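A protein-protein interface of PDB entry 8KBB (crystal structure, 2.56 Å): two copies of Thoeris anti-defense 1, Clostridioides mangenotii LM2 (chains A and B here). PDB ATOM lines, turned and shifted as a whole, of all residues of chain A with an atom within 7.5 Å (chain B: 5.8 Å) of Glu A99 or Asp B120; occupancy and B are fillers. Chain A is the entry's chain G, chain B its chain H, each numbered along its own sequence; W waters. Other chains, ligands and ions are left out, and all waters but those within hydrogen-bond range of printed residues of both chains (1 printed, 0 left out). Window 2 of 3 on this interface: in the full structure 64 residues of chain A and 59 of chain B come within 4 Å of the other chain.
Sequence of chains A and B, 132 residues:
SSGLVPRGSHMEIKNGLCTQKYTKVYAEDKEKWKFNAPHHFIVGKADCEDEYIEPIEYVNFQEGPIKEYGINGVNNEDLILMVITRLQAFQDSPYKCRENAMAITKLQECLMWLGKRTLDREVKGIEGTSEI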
ATOM      1  N   LEU A  87       3.228  29.206  -0.620  1.00  0.00           N
ATOM      2  CA  LEU A  87       3.233  28.520   0.667  1.00  0.00           C
ATOM      3  C   LEU A  87       3.110  29.515   1.819  1.00  0.00           C
ATOM      4  O   LEU A  87       2.396  29.266   2.800  1.00  0.00           O
ATOM      5  CB  LEU A  87       4.495  27.670   0.807  1.00  0.00           C
ATOM      6  CG  LEU A  87       4.550  26.406  -0.063  1.00  0.00           C
ATOM      7  CD1 LEU A  87       5.836  25.603   0.161  1.00  0.00           C
ATOM      8  CD2 LEU A  87       3.337  25.517   0.174  1.00  0.00           C
ATOM      9  N   GLN A  91       0.331  29.849   4.755  1.00  0.00           N
ATOM     10  CA  GLN A  91       0.632  29.930   6.182  1.00  0.00           C
ATOM     11  C   GLN A  91      -0.110  31.086   6.829  1.00  0.00           C
ATOM     12  O   GLN A  91      -0.517  30.995   7.993  1.00  0.00           O
ATOM     13  CB  GLN A  91       2.136  30.075   6.410  1.00  0.00           C
ATOM     14  CG  GLN A  91       2.923  28.804   6.174  1.00  0.00           C
ATOM     15  CD  GLN A  91       2.521  27.682   7.102  1.00  0.00           C
ATOM     16  OE1 GLN A  91       1.550  26.972   6.848  1.00  0.00           O
ATOM     17  NE2 GLN A  91       3.267  27.508   8.183  1.00  0.00           N
ATOM     18  N   LYS A  96      -2.715  27.233   7.717  1.00  0.00           N
ATOM     19  CA  LYS A  96      -1.391  27.211   8.318  1.00  0.00           C
ATOM     20  C   LYS A  96      -1.121  25.842   8.918  1.00  0.00           C
ATOM     21  O   LYS A  96      -1.978  25.275   9.594  1.00  0.00           O
ATOM     22  CB  LYS A  96      -1.321  28.293   9.395  1.00  0.00           C
ATOM     23  CG  LYS A  96       0.018  28.467  10.064  1.00  0.00           C
ATOM     24  CD  LYS A  96       0.099  29.840  10.725  1.00  0.00           C
ATOM     25  CE  LYS A  96       1.536  30.244  10.996  1.00  0.00           C
ATOM     26  NZ  LYS A  96       1.924  29.937  12.397  1.00  0.00           N
ATOM     27  N   CYS A  97       0.059  25.297   8.641  1.00  0.00           N
ATOM     28  CA  CYS A  97       0.393  23.964   9.121  1.00  0.00           C
ATOM     29  C   CYS A  97       1.903  23.810   9.130  1.00  0.00           C
ATOM     30  O   CYS A  97       2.624  24.517   8.420  1.00  0.00           O
ATOM     31  CB  CYS A  97      -0.242  22.871   8.263  1.00  0.00           C
ATOM     32  SG  CYS A  97       0.472  22.742   6.611  1.00  0.00           S
ATOM     33  N   ARG A  98       2.367  22.853   9.938  1.00  0.00           N
ATOM     34  CA  ARG A  98       3.797  22.662  10.146  1.00  0.00           C
ATOM     35  C   ARG A  98       4.492  22.166   8.881  1.00  0.00           C
ATOM     36  O   ARG A  98       5.640  22.543   8.607  1.00  0.00           O
ATOM     37  CB  ARG A  98       4.010  21.679  11.290  1.00  0.00           C
ATOM     38  CG  ARG A  98       5.451  21.390  11.603  1.00  0.00           C
ATOM     39  CD  ARG A  98       5.566  20.612  12.896  1.00  0.00           C
ATOM     40  NE  ARG A  98       6.801  19.836  12.944  1.00  0.00           N
ATOM     41  CZ  ARG A  98       6.885  18.538  12.674  1.00  0.00           C
ATOM     42  NH1 ARG A  98       5.794  17.852  12.338  1.00  0.00           N
ATOM     43  NH2 ARG A  98       8.063  17.929  12.744  1.00  0.00           N
ATOM     44  N   GLU A  99       3.818  21.312   8.103  1.00  0.00           N
ATOM     45  CA  GLU A  99       4.413  20.809   6.869  1.00  0.00           C
ATOM     46  C   GLU A  99       4.743  21.946   5.910  1.00  0.00           C
ATOM     47  O   GLU A  99       5.816  21.960   5.292  1.00  0.00           O
ATOM     48  CB  GLU A  99       3.477  19.796   6.216  1.00  0.00           C
ATOM     49  CG  GLU A  99       3.438  18.447   6.931  1.00  0.00           C
ATOM     50  CD  GLU A  99       2.583  18.455   8.192  1.00  0.00           C
ATOM     51  OE1 GLU A  99       2.608  17.452   8.933  1.00  0.00           O
ATOM     52  OE2 GLU A  99       1.886  19.459   8.440  1.00  0.00           O
ATOM     53  N   ASN A 100       3.840  22.919   5.782  1.00  0.00           N
ATOM     54  CA  ASN A 100       4.113  24.062   4.918  1.00  0.00           C
ATOM     55  C   ASN A 100       5.297  24.873   5.437  1.00  0.00           C
ATOM     56  O   ASN A 100       6.096  25.391   4.648  1.00  0.00           O
ATOM     57  CB  ASN A 100       2.877  24.952   4.808  1.00  0.00           C
ATOM     58  CG  ASN A 100       1.815  24.385   3.887  1.00  0.00           C
ATOM     59  OD1 ASN A 100       2.036  23.405   3.165  1.00  0.00           O
ATOM     60  ND2 ASN A 100       0.637  25.015   3.908  1.00  0.00           N
ATOM     61  N   ALA A 101       5.414  25.009   6.762  1.00  0.00           N
ATOM     62  CA  ALA A 101       6.545  25.731   7.331  1.00  0.00           C
ATOM     63  C   ALA A 101       7.860  25.021   7.022  1.00  0.00           C
ATOM     64  O   ALA A 101       8.849  25.666   6.646  1.00  0.00           O
ATOM     65  CB  ALA A 101       6.356  25.900   8.838  1.00  0.00           C
ATOM     66  N   MET A 102       7.878  23.694   7.145  1.00  0.00           N
ATOM     67  CA  MET A 102       9.074  22.936   6.798  1.00  0.00           C
ATOM     68  C   MET A 102       9.412  23.090   5.322  1.00  0.00           C
ATOM     69  O   MET A 102      10.588  23.214   4.959  1.00  0.00           O
ATOM     70  CB  MET A 102       8.887  21.460   7.145  1.00  0.00           C
ATOM     71  CG  MET A 102       8.839  21.208   8.624  1.00  0.00           C
ATOM     72  SD  MET A 102      10.343  21.763   9.446  1.00  0.00           S
ATOM     73  CE  MET A 102      11.616  21.068   8.365  1.00  0.00           C
ATOM     74  N   ALA A 103       8.397  23.095   4.456  1.00  0.00           N
ATOM     75  CA  ALA A 103       8.673  23.188   3.026  1.00  0.00           C
ATOM     76  C   ALA A 103       9.191  24.571   2.663  1.00  0.00           C
ATOM     77  O   ALA A 103      10.084  24.699   1.818  1.00  0.00           O
ATOM     78  CB  ALA A 103       7.426  22.830   2.214  1.00  0.00           C
ATOM     79  N   ILE A 104       8.656  25.618   3.297  1.00  0.00           N
ATOM     80  CA  ILE A 104       9.198  26.957   3.083  1.00  0.00           C
ATOM     81  C   ILE A 104      10.653  27.000   3.512  1.00  0.00           C
ATOM     82  O   ILE A 104      11.509  27.585   2.835  1.00  0.00           O
ATOM     83  CB  ILE A 104       8.376  28.014   3.836  1.00  0.00           C
ATOM     84  CG1 ILE A 104       7.005  28.206   3.192  1.00  0.00           C
ATOM     85  CG2 ILE A 104       9.147  29.341   3.883  1.00  0.00           C
ATOM     86  CD1 ILE A 104       5.948  28.760   4.134  1.00  0.00           C
ATOM     87  N   THR A 105      10.955  26.410   4.664  1.00  0.00           N
ATOM     88  CA  THR A 105      12.335  26.436   5.112  1.00  0.00           C
ATOM     89  C   THR A 105      13.234  25.732   4.104  1.00  0.00           C
ATOM     90  O   THR A 105      14.315  26.231   3.769  1.00  0.00           O
ATOM     91  CB  THR A 105      12.449  25.819   6.505  1.00  0.00           C
ATOM     92  OG1 THR A 105      11.803  26.687   7.430  1.00  0.00           O
ATOM     93  CG2 THR A 105      13.911  25.703   6.917  1.00  0.00           C
ATOM     94  N   LYS A 106      12.787  24.588   3.581  1.00  0.00           N
ATOM     95  CA  LYS A 106      13.594  23.882   2.592  1.00  0.00           C
ATOM     96  C   LYS A 106      13.802  24.738   1.345  1.00  0.00           C
ATOM     97  O   LYS A 106      14.918  24.827   0.825  1.00  0.00           O
ATOM     98  CB  LYS A 106      12.945  22.545   2.220  1.00  0.00           C
ATOM     99  CG  LYS A 106      12.817  21.518   3.353  1.00  0.00           C
ATOM    100  CD  LYS A 106      14.037  21.452   4.258  1.00  0.00           C
ATOM    101  CE  LYS A 106      13.889  20.284   5.239  1.00  0.00           C
ATOM    102  NZ  LYS A 106      15.138  19.826   5.936  1.00  0.00           N
ATOM    103  N   TRP B 113       7.976  16.944   2.614  1.00  0.00           N
ATOM    104  CA  TRP B 113       7.100  17.583   3.601  1.00  0.00           C
ATOM    105  C   TRP B 113       5.726  17.920   3.016  1.00  0.00           C
ATOM    106  O   TRP B 113       4.690  17.709   3.674  1.00  0.00           O
ATOM    107  CB  TRP B 113       7.769  18.835   4.168  1.00  0.00           C
ATOM    108  CG  TRP B 113       8.797  18.503   5.212  1.00  0.00           C
ATOM    109  CD1 TRP B 113      10.152  18.541   5.072  1.00  0.00           C
ATOM    110  CD2 TRP B 113       8.544  18.060   6.546  1.00  0.00           C
ATOM    111  NE1 TRP B 113      10.762  18.157   6.239  1.00  0.00           N
ATOM    112  CE2 TRP B 113       9.793  17.861   7.164  1.00  0.00           C
ATOM    113  CE3 TRP B 113       7.382  17.819   7.282  1.00  0.00           C
ATOM    114  CZ2 TRP B 113       9.910  17.418   8.484  1.00  0.00           C
ATOM    115  CZ3 TRP B 113       7.501  17.385   8.590  1.00  0.00           C
ATOM    116  CH2 TRP B 113       8.754  17.186   9.178  1.00  0.00           C
ATOM    117  N   LEU B 114       5.688  18.448   1.784  1.00  0.00           N
ATOM    118  CA  LEU B 114       4.392  18.676   1.140  1.00  0.00           C
ATOM    119  C   LEU B 114       3.619  17.368   0.994  1.00  0.00           C
ATOM    120  O   LEU B 114       2.398  17.298   1.251  1.00  0.00           O
ATOM    121  CB  LEU B 114       4.598  19.333  -0.221  1.00  0.00           C
ATOM    122  CG  LEU B 114       5.326  20.670  -0.215  1.00  0.00           C
ATOM    123  CD1 LEU B 114       5.741  21.047  -1.623  1.00  0.00           C
ATOM    124  CD2 LEU B 114       4.416  21.737   0.382  1.00  0.00           C
ATOM    125  N   GLY B 115       4.326  16.304   0.614  1.00  0.00           N
ATOM    126  CA  GLY B 115       3.686  15.015   0.501  1.00  0.00           C
ATOM    127  C   GLY B 115       3.162  14.525   1.832  1.00  0.00           C
ATOM    128  O   GLY B 115       2.139  13.846   1.885  1.00  0.00           O
ATOM    129  N   LYS B 116       3.873  14.844   2.919  1.00  0.00           N
ATOM    130  CA  LYS B 116       3.416  14.439   4.242  1.00  0.00           C
ATOM    131  C   LYS B 116       2.095  15.090   4.580  1.00  0.00           C
ATOM    132  O   LYS B 116       1.210  14.440   5.147  1.00  0.00           O
ATOM    133  CB  LYS B 116       4.442  14.782   5.314  1.00  0.00           C
ATOM    134  CG  LYS B 116       3.949  14.471   6.727  1.00  0.00           C
ATOM    135  CD  LYS B 116       4.957  14.896   7.788  1.00  0.00           C
ATOM    136  CE  LYS B 116       4.510  14.522   9.196  1.00  0.00           C
ATOM    137  NZ  LYS B 116       3.223  15.152   9.614  1.00  0.00           N
ATOM    138  N   ARG B 117       1.948  16.383   4.270  1.00  0.00           N
ATOM    139  CA  ARG B 117       0.628  16.986   4.460  1.00  0.00           C
ATOM    140  C   ARG B 117      -0.434  16.139   3.758  1.00  0.00           C
ATOM    141  O   ARG B 117      -1.454  15.764   4.358  1.00  0.00           O
ATOM    142  CB  ARG B 117       0.572  18.442   3.965  1.00  0.00           C
ATOM    143  CG  ARG B 117      -0.867  19.016   4.077  1.00  0.00           C
ATOM    144  CD  ARG B 117      -1.033  20.542   3.964  1.00  0.00           C
ATOM    145  NE  ARG B 117      -1.109  21.058   2.594  1.00  0.00           N
ATOM    146  CZ  ARG B 117      -1.655  22.233   2.269  1.00  0.00           C
ATOM    147  NH1 ARG B 117      -2.187  23.004   3.212  1.00  0.00           N
ATOM    148  NH2 ARG B 117      -1.685  22.640   1.001  1.00  0.00           N
ATOM    149  N   THR B 118      -0.174  15.778   2.493  1.00  0.00           N
ATOM    150  CA  THR B 118      -1.166  14.984   1.756  1.00  0.00           C
ATOM    151  C   THR B 118      -1.421  13.615   2.405  1.00  0.00           C
ATOM    152  O   THR B 118      -2.574  13.209   2.589  1.00  0.00           O
ATOM    153  CB  THR B 118      -0.736  14.810   0.301  1.00  0.00           C
ATOM    154  OG1 THR B 118      -0.727  16.088  -0.349  1.00  0.00           O
ATOM    155  CG2 THR B 118      -1.697  13.887  -0.423  1.00  0.00           C
ATOM    156  N   LEU B 119      -0.355  12.874   2.723  1.00  0.00           N
ATOM    157  CA  LEU B 119      -0.492  11.523   3.270  1.00  0.00           C
ATOM    158  C   LEU B 119      -1.206  11.536   4.616  1.00  0.00           C
ATOM    159  O   LEU B 119      -1.952  10.599   4.950  1.00  0.00           O
ATOM    160  CB  LEU B 119       0.888  10.872   3.425  1.00  0.00           C
ATOM    161  CG  LEU B 119       1.708  10.491   2.187  1.00  0.00           C
ATOM    162  CD1 LEU B 119       2.931   9.653   2.562  1.00  0.00           C
ATOM    163  CD2 LEU B 119       0.853   9.749   1.174  1.00  0.00           C
ATOM    164  N   ASP B 120      -0.979  12.586   5.405  1.00  0.00           N
ATOM    165  CA  ASP B 120      -1.699  12.749   6.656  1.00  0.00           C
ATOM    166  C   ASP B 120      -3.182  12.957   6.389  1.00  0.00           C
ATOM    167  O   ASP B 120      -4.030  12.328   7.032  1.00  0.00           O
ATOM    168  CB  ASP B 120      -1.110  13.922   7.443  1.00  0.00           C
ATOM    169  CG  ASP B 120       0.209  13.573   8.137  1.00  0.00           C
ATOM    170  OD1 ASP B 120       0.683  12.414   8.014  1.00  0.00           O
ATOM    171  OD2 ASP B 120       0.778  14.471   8.800  1.00  0.00           O
ATOM    172  N   ARG B 121      -3.516  13.814   5.415  1.00  0.00           N
ATOM    173  CA  ARG B 121      -4.928  14.009   5.087  1.00  0.00           C
ATOM    174  C   ARG B 121      -5.556  12.737   4.511  1.00  0.00           C
ATOM    175  O   ARG B 121      -6.781  12.586   4.568  1.00  0.00           O
ATOM    176  CB  ARG B 121      -5.103  15.202   4.132  1.00  0.00           C
ATOM    177  CG  ARG B 121      -4.621  16.479   4.794  1.00  0.00           C
ATOM    178  CD  ARG B 121      -4.759  17.787   4.007  1.00  0.00           C
ATOM    179  NE  ARG B 121      -6.139  18.181   3.867  1.00  0.00           N
ATOM    180  CZ  ARG B 121      -6.767  18.959   4.756  1.00  0.00           C
ATOM    181  NH1 ARG B 121      -6.168  19.334   5.894  1.00  0.00           N
ATOM    182  NH2 ARG B 121      -8.033  19.319   4.536  1.00  0.00           N
ATOM    183  N   GLU B 122      -4.744  11.818   3.974  1.00  0.00           N
ATOM    184  CA  GLU B 122      -5.234  10.478   3.639  1.00  0.00           C
ATOM    185  C   GLU B 122      -5.602   9.695   4.888  1.00  0.00           C
ATOM    186  O   GLU B 122      -6.739   9.237   5.037  1.00  0.00           O
ATOM    187  CB  GLU B 122      -4.192   9.685   2.863  1.00  0.00           C
ATOM    188  CG  GLU B 122      -3.992  10.024   1.422  1.00  0.00           C
ATOM    189  CD  GLU B 122      -3.101   8.983   0.780  1.00  0.00           C
ATOM    190  OE1 GLU B 122      -2.890   7.933   1.427  1.00  0.00           O
ATOM    191  OE2 GLU B 122      -2.603   9.205  -0.344  1.00  0.00           O
ATOM    192  N   VAL B 123      -4.626   9.483   5.777  1.00  0.00           N
ATOM    193  CA  VAL B 123      -4.875   8.712   6.993  1.00  0.00           C
ATOM    194  C   VAL B 123      -6.033   9.301   7.806  1.00  0.00           C
ATOM    195  O   VAL B 123      -6.669   8.590   8.596  1.00  0.00           O
ATOM    196  CB  VAL B 123      -3.559   8.614   7.805  1.00  0.00           C
ATOM    197  CG1 VAL B 123      -3.809   8.176   9.231  1.00  0.00           C
ATOM    198  CG2 VAL B 123      -2.588   7.645   7.126  1.00  0.00           C
ATOM    199  N   LYS B 124      -6.353  10.578   7.587  1.00  0.00           N
ATOM    200  CA  LYS B 124      -7.506  11.243   8.187  1.00  0.00           C
ATOM    201  C   LYS B 124      -8.757  11.204   7.307  1.00  0.00           C
ATOM    202  O   LYS B 124      -9.845  11.534   7.791  1.00  0.00           O
ATOM    203  CB  LYS B 124      -7.155  12.704   8.498  1.00  0.00           C
ATOM    204  CG  LYS B 124      -7.634  13.202   9.845  1.00  0.00           C
ATOM    205  CD  LYS B 124      -7.189  14.640  10.064  1.00  0.00           C
ATOM    206  CE  LYS B 124      -5.712  14.718  10.410  1.00  0.00           C
ATOM    207  NZ  LYS B 124      -5.382  15.986  11.110  1.00  0.00           N
ATOM    208  N   GLY B 125      -8.627  10.839   6.030  1.00  0.00           N
ATOM    209  CA  GLY B 125      -9.764  10.633   5.153  1.00  0.00           C
ATOM    210  C   GLY B 125     -10.273  11.852   4.410  1.00  0.00           C
ATOM    211  O   GLY B 125     -11.236  11.727   3.640  1.00  0.00           O
HETATM  212  O   HOH W   1       0.759  22.574   0.488  1.00  0.00           O
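Leu B114 touches Leu A87. Arg B117 touches Cys A97 (CD to SG, 3.8 Å). CH2 of Trp B113 touches NH2 of Arg A98, at 3.7 Å. Glu A99 touches Trp B113 (CB to O, 3.5 Å). CG of Glu A99 touches N of Arg B117, 3.7 Å away. Glu A99 touches Asp B120. Asn A100 touches Arg B117. Met A102 touches Trp B113. CD2 of Leu B114 touches CB of Ala A103 (3.7 Å). NE1 of Trp B113 touches CE of Lys A106, 3.9 Å away.
Printed residues of chain A that touch a printed residue of chain B: Leu A87, Cys A97, Arg A98, Glu A99, Asn A100, Met A102, Ala A103 and Lys A106. Of the 13 printed residues of chain B, 5 touch a printed residue of chain A. Printed residues of chain B that touch a printed residue of chain A: Trp B113, Leu B114, Lys B116, Arg B117 and Asp B120. Hydrophobic or aromatic side chains of chain B that line the printed part of chain A: Trp B113 and Leu B114. Among the printed residues, 11 pairs touch across the chains. Among the printed residues, Asp or Glu carboxylates within 4 Å of a Lys or Arg side-chain nitrogen of the other chain: Glu A99 with Lys B116 (2.5 Å).
Water W1 lies within hydrogen-bond range of NH2 of Arg B117 and OD1 of Asn A100.
The side-chain amino group of Lys B116 is in salt-bridge range of the side-chain carboxylate of Asp B120 (2.7 Å). The side-chain sulfur (SG) of Cys A97 sits close to the backbone NH (N) of Asn A100, 3.5 Å away. The side-chain amide oxygen (OE1) of Gln A91 sits at hydrogen-bond distance from the backbone NH (N) of Cys A97 (2.9 Å).
No position is printed for both chains. Of the 11 pairs that touch across the chains among the printed residues, none has its exchanged pair printed and touching as well.
Of chain B, only Trp B113, Lys B116, Arg B117 and Asp B120 come within 4 Å of Glu A99. Asp B120 touches just one residue of chain A: Glu A99 (3.5 Å). Printed residues of chain A within 4 Å of Arg B117: Cys A97, Glu A99 and Asn A100. Printed residues of chain B within 4 Å of Met A102: Trp B113 (3.5 Å). Of the printed residues of chain A, Lys B116 touches Glu A99. Arg B121 touches none of the printed residues of chain A. Glu B122 touches none of the printed residues of chain A. The nearest residue of chain B that does not touch Glu A99 is Leu B114 (5.0 Å). The nearest residue of chain A that does not touch Asp B120 is Arg A98 (7.0 Å). The nearest printed residue of chain B that does not touch Asn A100 is Leu B114 (4.02 Å).
The side-chain amino group of Lys B116 lies within salt-bridge range of the side-chain carboxylate of Glu A99 (2.5 Å).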
